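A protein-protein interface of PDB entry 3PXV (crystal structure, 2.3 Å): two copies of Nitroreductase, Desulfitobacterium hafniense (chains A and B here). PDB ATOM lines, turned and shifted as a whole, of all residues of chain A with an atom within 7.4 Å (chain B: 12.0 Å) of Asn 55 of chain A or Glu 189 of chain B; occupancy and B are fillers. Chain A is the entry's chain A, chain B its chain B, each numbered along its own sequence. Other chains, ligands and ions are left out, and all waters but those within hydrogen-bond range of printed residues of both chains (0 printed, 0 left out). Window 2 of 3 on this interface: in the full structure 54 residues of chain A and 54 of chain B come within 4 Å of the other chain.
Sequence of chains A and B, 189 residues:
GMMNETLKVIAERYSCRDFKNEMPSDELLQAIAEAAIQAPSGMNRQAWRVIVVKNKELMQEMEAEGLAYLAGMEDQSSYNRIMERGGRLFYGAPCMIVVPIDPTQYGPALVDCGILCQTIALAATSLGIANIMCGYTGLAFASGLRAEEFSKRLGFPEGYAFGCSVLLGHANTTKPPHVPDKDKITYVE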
ATOM      1  N   MET A  23      -0.001  -4.786   8.354  1.00  0.00           N
ATOM      2  CA  MET A  23       0.817  -5.372   7.303  1.00  0.00           C
ATOM      3  C   MET A  23       0.709  -6.898   7.227  1.00  0.00           C
ATOM      4  O   MET A  23       0.971  -7.592   8.208  1.00  0.00           O
ATOM      5  CB  MET A  23       2.295  -4.995   7.552  1.00  0.00           C
ATOM      6  CG  MET A  23       3.252  -5.367   6.411  1.00  0.00           C
ATOM      7  SD  MET A  23       2.923  -4.332   4.827  1.00  0.00           S
ATOM      8  CE  MET A  23       3.588  -2.642   5.566  1.00  0.00           C
ATOM      9  N   ASP A  26       5.276 -11.426   6.104  1.00  0.00           N
ATOM     10  CA  ASP A  26       6.217 -11.660   5.026  1.00  0.00           C
ATOM     11  C   ASP A  26       5.878 -12.985   4.334  1.00  0.00           C
ATOM     12  O   ASP A  26       5.920 -13.087   3.103  1.00  0.00           O
ATOM     13  CB  ASP A  26       7.655 -11.655   5.560  1.00  0.00           C
ATOM     14  CG  ASP A  26       8.170 -10.229   5.871  1.00  0.00           C
ATOM     15  OD1 ASP A  26       7.587  -9.232   5.356  1.00  0.00           O
ATOM     16  OD2 ASP A  26       9.189 -10.112   6.594  1.00  0.00           O
ATOM     17  N   LEU A  29       3.071 -12.393   1.849  1.00  0.00           N
ATOM     18  CA  LEU A  29       3.568 -11.578   0.751  1.00  0.00           C
ATOM     19  C   LEU A  29       4.436 -12.405  -0.192  1.00  0.00           C
ATOM     20  O   LEU A  29       4.301 -12.301  -1.403  1.00  0.00           O
ATOM     21  CB  LEU A  29       4.357 -10.363   1.264  1.00  0.00           C
ATOM     22  CG  LEU A  29       3.509  -9.292   1.944  1.00  0.00           C
ATOM     23  CD1 LEU A  29       4.385  -8.167   2.526  1.00  0.00           C
ATOM     24  CD2 LEU A  29       2.490  -8.753   0.937  1.00  0.00           C
ATOM     25  N   VAL A  52       7.367  -5.702  -4.382  1.00  0.00           N
ATOM     26  CA  VAL A  52       6.523  -5.653  -3.182  1.00  0.00           C
ATOM     27  C   VAL A  52       6.893  -4.410  -2.382  1.00  0.00           C
ATOM     28  O   VAL A  52       7.970  -4.318  -1.817  1.00  0.00           O
ATOM     29  CB  VAL A  52       6.660  -6.917  -2.352  1.00  0.00           C
ATOM     30  CG1 VAL A  52       5.718  -6.859  -1.182  1.00  0.00           C
ATOM     31  CG2 VAL A  52       6.403  -8.141  -3.256  1.00  0.00           C
ATOM     32  N   VAL A  53       5.965  -3.468  -2.350  1.00  0.00           N
ATOM     33  CA  VAL A  53       6.157  -2.170  -1.741  1.00  0.00           C
ATOM     34  C   VAL A  53       5.511  -2.098  -0.378  1.00  0.00           C
ATOM     35  O   VAL A  53       4.273  -2.092  -0.277  1.00  0.00           O
ATOM     36  CB  VAL A  53       5.535  -1.090  -2.645  1.00  0.00           C
ATOM     37  CG1 VAL A  53       5.636   0.274  -1.990  1.00  0.00           C
ATOM     38  CG2 VAL A  53       6.207  -1.117  -4.011  1.00  0.00           C
ATOM     39  N   LYS A  54       6.346  -2.055   0.661  1.00  0.00           N
ATOM     40  CA  LYS A  54       5.883  -1.968   2.047  1.00  0.00           C
ATOM     41  C   LYS A  54       6.140  -0.604   2.676  1.00  0.00           C
ATOM     42  O   LYS A  54       5.704  -0.355   3.795  1.00  0.00           O
ATOM     43  CB  LYS A  54       6.574  -3.032   2.904  1.00  0.00           C
ATOM     44  CG  LYS A  54       6.143  -4.435   2.575  1.00  0.00           C
ATOM     45  CD  LYS A  54       7.064  -5.487   3.137  1.00  0.00           C
ATOM     46  CE  LYS A  54       7.135  -5.469   4.658  1.00  0.00           C
ATOM     47  NZ  LYS A  54       8.134  -6.484   5.052  1.00  0.00           N
ATOM     48  N   ASN A  55       6.815   0.281   1.951  1.00  0.00           N
ATOM     49  CA  ASN A  55       7.212   1.595   2.479  1.00  0.00           C
ATOM     50  C   ASN A  55       6.042   2.573   2.486  1.00  0.00           C
ATOM     51  O   ASN A  55       5.589   3.020   1.436  1.00  0.00           O
ATOM     52  CB  ASN A  55       8.393   2.132   1.677  1.00  0.00           C
ATOM     53  CG  ASN A  55       8.954   3.417   2.235  1.00  0.00           C
ATOM     54  OD1 ASN A  55       8.412   4.481   2.022  1.00  0.00           O
ATOM     55  ND2 ASN A  55      10.098   3.329   2.878  1.00  0.00           N
ATOM     56  N   LYS A  56       5.577   2.908   3.682  1.00  0.00           N
ATOM     57  CA  LYS A  56       4.428   3.783   3.848  1.00  0.00           C
ATOM     58  C   LYS A  56       4.622   5.174   3.234  1.00  0.00           C
ATOM     59  O   LYS A  56       3.732   5.682   2.555  1.00  0.00           O
ATOM     60  CB  LYS A  56       4.075   3.921   5.340  1.00  0.00           C
ATOM     61  CG  LYS A  56       2.704   4.530   5.609  1.00  0.00           C
ATOM     62  CD  LYS A  56       2.480   4.741   7.101  1.00  0.00           C
ATOM     63  CE  LYS A  56       1.027   5.055   7.413  1.00  0.00           C
ATOM     64  NZ  LYS A  56       0.862   5.398   8.866  1.00  0.00           N
ATOM     65  N   GLU A  57       5.772   5.784   3.488  1.00  0.00           N
ATOM     66  CA  GLU A  57       6.065   7.126   2.981  1.00  0.00           C
ATOM     67  C   GLU A  57       6.075   7.148   1.426  1.00  0.00           C
ATOM     68  O   GLU A  57       5.530   8.083   0.825  1.00  0.00           O
ATOM     69  CB  GLU A  57       7.351   7.678   3.639  1.00  0.00           C
ATOM     70  CG  GLU A  57       7.980   8.954   3.028  1.00  0.00           C
ATOM     71  CD  GLU A  57       7.095  10.210   3.102  1.00  0.00           C
ATOM     72  OE1 GLU A  57       6.039  10.211   3.777  1.00  0.00           O
ATOM     73  OE2 GLU A  57       7.473  11.216   2.472  1.00  0.00           O
ATOM     74  N   LEU A  58       6.624   6.118   0.776  1.00  0.00           N
ATOM     75  CA  LEU A  58       6.610   6.064  -0.699  1.00  0.00           C
ATOM     76  C   LEU A  58       5.147   6.004  -1.192  1.00  0.00           C
ATOM     77  O   LEU A  58       4.743   6.780  -2.073  1.00  0.00           O
ATOM     78  CB  LEU A  58       7.422   4.860  -1.216  1.00  0.00           C
ATOM     79  CG  LEU A  58       7.582   4.685  -2.734  1.00  0.00           C
ATOM     80  CD1 LEU A  58       8.064   5.967  -3.384  1.00  0.00           C
ATOM     81  CD2 LEU A  58       8.527   3.517  -3.118  1.00  0.00           C
ATOM     82  N   MET A  59       4.337   5.119  -0.600  1.00  0.00           N
ATOM     83  CA  MET A  59       2.928   5.039  -0.993  1.00  0.00           C
ATOM     84  C   MET A  59       2.163   6.340  -0.746  1.00  0.00           C
ATOM     85  O   MET A  59       1.390   6.756  -1.577  1.00  0.00           O
ATOM     86  CB  MET A  59       2.228   3.891  -0.291  1.00  0.00           C
ATOM     87  CG  MET A  59       2.809   2.560  -0.720  1.00  0.00           C
ATOM     88  SD  MET A  59       1.938   1.104   0.086  1.00  0.00           S
ATOM     89  CE  MET A  59       0.172   1.351  -0.619  1.00  0.00           C
ATOM     90  N   GLN A  60       2.392   6.983   0.387  1.00  0.00           N
ATOM     91  CA  GLN A  60       1.715   8.225   0.698  1.00  0.00           C
ATOM     92  C   GLN A  60       2.055   9.333  -0.291  1.00  0.00           C
ATOM     93  O   GLN A  60       1.220  10.159  -0.601  1.00  0.00           O
ATOM     94  CB  GLN A  60       2.067   8.694   2.125  1.00  0.00           C
ATOM     95  CG  GLN A  60       1.385   7.922   3.284  1.00  0.00           C
ATOM     96  CD  GLN A  60       1.833   8.425   4.676  1.00  0.00           C
ATOM     97  OE1 GLN A  60       2.985   8.820   4.872  1.00  0.00           O
ATOM     98  NE2 GLN A  60       0.930   8.383   5.636  1.00  0.00           N
ATOM     99  N   GLU A  61       3.298   9.370  -0.751  1.00  0.00           N
ATOM    100  CA  GLU A  61       3.724  10.381  -1.711  1.00  0.00           C
ATOM    101  C   GLU A  61       3.201  10.093  -3.118  1.00  0.00           C
ATOM    102  O   GLU A  61       2.870  11.015  -3.854  1.00  0.00           O
ATOM    103  CB  GLU A  61       5.250  10.493  -1.755  1.00  0.00           C
ATOM    104  CG  GLU A  61       5.921  11.111  -0.536  1.00  0.00           C
ATOM    105  CD  GLU A  61       7.436  11.261  -0.759  1.00  0.00           C
ATOM    106  OE1 GLU A  61       7.832  11.678  -1.869  1.00  0.00           O
ATOM    107  OE2 GLU A  61       8.229  10.953   0.157  1.00  0.00           O
ATOM    108  N   PRO A  94      -1.850  -0.983   3.112  1.00  0.00           N
ATOM    109  CA  PRO A  94      -0.571  -0.824   3.730  1.00  0.00           C
ATOM    110  C   PRO A  94       0.593  -1.292   2.873  1.00  0.00           C
ATOM    111  O   PRO A  94       1.744  -1.151   3.292  1.00  0.00           O
ATOM    112  CB  PRO A  94      -0.681  -1.735   4.966  1.00  0.00           C
ATOM    113  CG  PRO A  94      -1.532  -2.831   4.511  1.00  0.00           C
ATOM    114  CD  PRO A  94      -2.573  -2.139   3.666  1.00  0.00           C
ATOM    115  N   CYS A  95       0.292  -1.960   1.768  1.00  0.00           N
ATOM    116  CA  CYS A  95       1.307  -2.433   0.855  1.00  0.00           C
ATOM    117  C   CYS A  95       0.719  -2.701  -0.500  1.00  0.00           C
ATOM    118  O   CYS A  95      -0.484  -2.750  -0.662  1.00  0.00           O
ATOM    119  CB  CYS A  95       1.997  -3.682   1.378  1.00  0.00           C
ATOM    120  SG  CYS A  95       1.186  -5.214   1.110  1.00  0.00           S
ATOM    121  N   MET A  96       1.580  -2.819  -1.491  1.00  0.00           N
ATOM    122  CA  MET A  96       1.130  -3.083  -2.844  1.00  0.00           C
ATOM    123  C   MET A  96       2.244  -3.718  -3.639  1.00  0.00           C
ATOM    124  O   MET A  96       3.400  -3.612  -3.267  1.00  0.00           O
ATOM    125  CB  MET A  96       0.678  -1.790  -3.535  1.00  0.00           C
ATOM    126  CG  MET A  96       1.788  -0.821  -3.850  1.00  0.00           C
ATOM    127  SD  MET A  96       1.119   0.700  -4.825  1.00  0.00           S
ATOM    128  CE  MET A  96       2.765   1.703  -5.037  1.00  0.00           C
ATOM    129  N   ARG A 153      13.087   4.954  -6.951  1.00  0.00           N
ATOM    130  CA  ARG A 153      12.755   4.617  -5.566  1.00  0.00           C
ATOM    131  C   ARG A 153      12.153   3.253  -5.476  1.00  0.00           C
ATOM    132  O   ARG A 153      12.354   2.571  -4.481  1.00  0.00           O
ATOM    133  CB  ARG A 153      11.842   5.668  -4.915  1.00  0.00           C
ATOM    134  CG  ARG A 153      12.576   6.976  -4.619  1.00  0.00           C
ATOM    135  CD  ARG A 153      11.640   8.099  -4.134  1.00  0.00           C
ATOM    136  NE  ARG A 153      11.073   7.915  -2.798  1.00  0.00           N
ATOM    137  CZ  ARG A 153      10.256   8.793  -2.200  1.00  0.00           C
ATOM    138  NH1 ARG A 153       9.894   9.927  -2.819  1.00  0.00           N
ATOM    139  NH2 ARG A 153       9.781   8.544  -0.978  1.00  0.00           N
ATOM    140  N   ILE B 185      11.556 -10.725  -8.221  1.00  0.00           N
ATOM    141  CA  ILE B 185      10.828 -10.230  -7.058  1.00  0.00           C
ATOM    142  C   ILE B 185      11.780  -9.449  -6.174  1.00  0.00           C
ATOM    143  O   ILE B 185      12.809  -9.996  -5.761  1.00  0.00           O
ATOM    144  CB  ILE B 185      10.341 -11.374  -6.151  1.00  0.00           C
ATOM    145  CG1 ILE B 185       9.309 -12.246  -6.869  1.00  0.00           C
ATOM    146  CG2 ILE B 185       9.799 -10.799  -4.845  1.00  0.00           C
ATOM    147  CD1 ILE B 185       9.107 -13.616  -6.209  1.00  0.00           C
ATOM    148  N   THR B 186      11.467  -8.181  -5.904  1.00  0.00           N
ATOM    149  CA  THR B 186      12.230  -7.401  -4.926  1.00  0.00           C
ATOM    150  C   THR B 186      11.236  -6.802  -3.939  1.00  0.00           C
ATOM    151  O   THR B 186      10.037  -6.800  -4.196  1.00  0.00           O
ATOM    152  CB  THR B 186      13.040  -6.265  -5.556  1.00  0.00           C
ATOM    153  OG1 THR B 186      12.182  -5.531  -6.428  1.00  0.00           O
ATOM    154  CG2 THR B 186      14.241  -6.801  -6.346  1.00  0.00           C
ATOM    155  N   TYR B 187      11.755  -6.297  -2.816  1.00  0.00           N
ATOM    156  CA  TYR B 187      10.954  -5.675  -1.781  1.00  0.00           C
ATOM    157  C   TYR B 187      11.399  -4.237  -1.527  1.00  0.00           C
ATOM    158  O   TYR B 187      12.571  -3.969  -1.475  1.00  0.00           O
ATOM    159  CB  TYR B 187      11.103  -6.471  -0.504  1.00  0.00           C
ATOM    160  CG  TYR B 187      10.369  -7.773  -0.523  1.00  0.00           C
ATOM    161  CD1 TYR B 187      10.861  -8.873  -1.222  1.00  0.00           C
ATOM    162  CD2 TYR B 187       9.190  -7.920   0.184  1.00  0.00           C
ATOM    163  CE1 TYR B 187      10.177 -10.072  -1.233  1.00  0.00           C
ATOM    164  CE2 TYR B 187       8.489  -9.122   0.177  1.00  0.00           C
ATOM    165  CZ  TYR B 187       8.986 -10.182  -0.527  1.00  0.00           C
ATOM    166  OH  TYR B 187       8.274 -11.346  -0.509  1.00  0.00           O
ATOM    167  N   VAL B 188      10.461  -3.304  -1.434  1.00  0.00           N
ATOM    168  CA  VAL B 188      10.803  -1.926  -1.088  1.00  0.00           C
ATOM    169  C   VAL B 188      10.247  -1.735   0.328  1.00  0.00           C
ATOM    170  O   VAL B 188       9.037  -1.543   0.521  1.00  0.00           O
ATOM    171  CB  VAL B 188      10.248  -0.934  -2.091  1.00  0.00           C
ATOM    172  CG1 VAL B 188      10.656   0.506  -1.701  1.00  0.00           C
ATOM    173  CG2 VAL B 188      10.749  -1.297  -3.496  1.00  0.00           C
ATOM    174  N   GLU B 189      11.140  -1.863   1.308  1.00  0.00           N
ATOM    175  CA  GLU B 189      10.779  -1.811   2.715  1.00  0.00           C
ATOM    176  C   GLU B 189      10.674  -0.363   3.178  1.00  0.00           C
ATOM    177  O   GLU B 189      11.392   0.519   2.675  1.00  0.00           O
ATOM    178  CB  GLU B 189      11.833  -2.532   3.583  1.00  0.00           C
ATOM    179  CG  GLU B 189      12.119  -4.000   3.259  1.00  0.00           C
ATOM    180  CD  GLU B 189      11.069  -4.982   3.773  1.00  0.00           C
ATOM    181  OE1 GLU B 189      10.211  -4.633   4.636  1.00  0.00           O
ATOM    182  OE2 GLU B 189      11.143  -6.138   3.309  1.00  0.00           O
ATOM    183  OXT GLU B 189       9.878  -0.068   4.079  1.00  0.00           O
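The side-chain amino group (NZ) of Lys 54 of chain A lies within salt-bridge range of the side-chain carboxylate (OD1) of Asp 26 of chain A, 2.8 Å away.
The backbone NH (N) of Val 53 of chain A sits at hydrogen-bond distance from the backbone carbonyl oxygen (O) of Met 96 of chain A, 2.7 Å away.
The backbone NH of Glu 57 of chain A is in hydrogen-bond range of the side-chain amide oxygen of Asn 55 of chain A (3.3 Å).
The side-chain amide oxygen (OD1) of Asn 55 of chain A is in hydrogen-bond range of the backbone NH (N) of Leu 58 of chain A, at 2.7 Å.
The side-chain carboxylate of Glu 61 of chain A is in salt-bridge range of the guanidinium group of Arg 153 of chain A (2.9 Å).
Among the printed residues, pairs that only touch across the chains: Val 52 of chain A with Tyr 187 of chain B (3.3 Å), Val 53 of chain A with Val 188 of chain B (3.7 Å), Arg 153 of chain A with Val 188 of chain B (3.9 Å), Leu 58 of chain A with Val 188 of chain B (3.95 Å) and Leu 29 of chain A with Tyr 187 of chain B (3.99 Å).
O of Thr 186 of chain B lies within hydrogen-bond range of N of Val 52 of chain A.
The backbone NH (N) of Val 188 of chain B sits at hydrogen-bond distance from the backbone carbonyl oxygen (O) of Val 52 of chain A (2.7 Å).
O of Val 188 of chain B lies within hydrogen-bond range of N of Lys 54 of chain A (2.7 Å).
NZ of Lys 54 of chain A is in salt-bridge range of OE1 of Glu 189 of chain B (2.8 Å).
The backbone carbonyl oxygen (O) of Val 188 of chain B sits at hydrogen-bond distance from the backbone NH (N) of Asn 55 of chain A (3.2 Å).
The side-chain amide nitrogen (ND2) of Asn 55 of chain A is in hydrogen-bond range of the chain-end carboxylate (O) of Glu 189 of chain B (3.1 Å).
No position is printed for both chains.
Of the 11 pairs that touch across the chains among the printed residues, none has its exchanged pair printed and touching as well.
Asn 55 of chain A touches just these residues of chain B: Val 188 and Glu 189.
Of chain A, only Lys 54 (2.8 Å) and Asn 55 (3.1 Å) come within 4 Å of Glu 189 of chain B.
Val 53 of chain A touches just one residue of chain B: Val 188.
Lys 54 of chain A touches two residues of chain B.
No residue of chain B comes within 4 Å of Glu 57 of chain A.
Leu 58 of chain A touches just one residue of chain B: Val 188.
No residue of chain B comes within 4 Å of Met 59 of chain A.
Printed residues of chain B within 4 Å of Leu 29 of chain A: Tyr 187.
Of the printed residues of chain A, Tyr 187 of chain B touches Leu 29 (3.99 Å) and Val 52 (3.3 Å).
Of the printed residues of chain A, Thr 186 of chain B touches Val 52.
Of the printed residues of chain A, Val 188 of chain B touches Val 52 (2.7 Å), Val 53 (3.7 Å), Lys 54 (2.7 Å), Asn 55 (3.2 Å), Leu 58 (3.95 Å) and Arg 153 (3.9 Å).
Of the printed residues of chain B, Val 52 of chain A touches Thr 186 (2.9 Å), Tyr 187 (3.3 Å) and Val 188 (2.7 Å).
The nearest residue of chain A that does not touch Glu 189 of chain B is Val 52 of chain A (5.1 Å).
The nearest printed residue of chain A that does not touch Tyr 187 of chain B is Lys 54 of chain A (4.4 Å).
Among the printed residues, 11 pairs touch across the chains.
Among the printed residues, Asp or Glu carboxylates within 4 Å of a Lys or Arg side-chain nitrogen of the other chain: Lys 54 of chain A with Glu 189 of chain B (2.8 Å).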
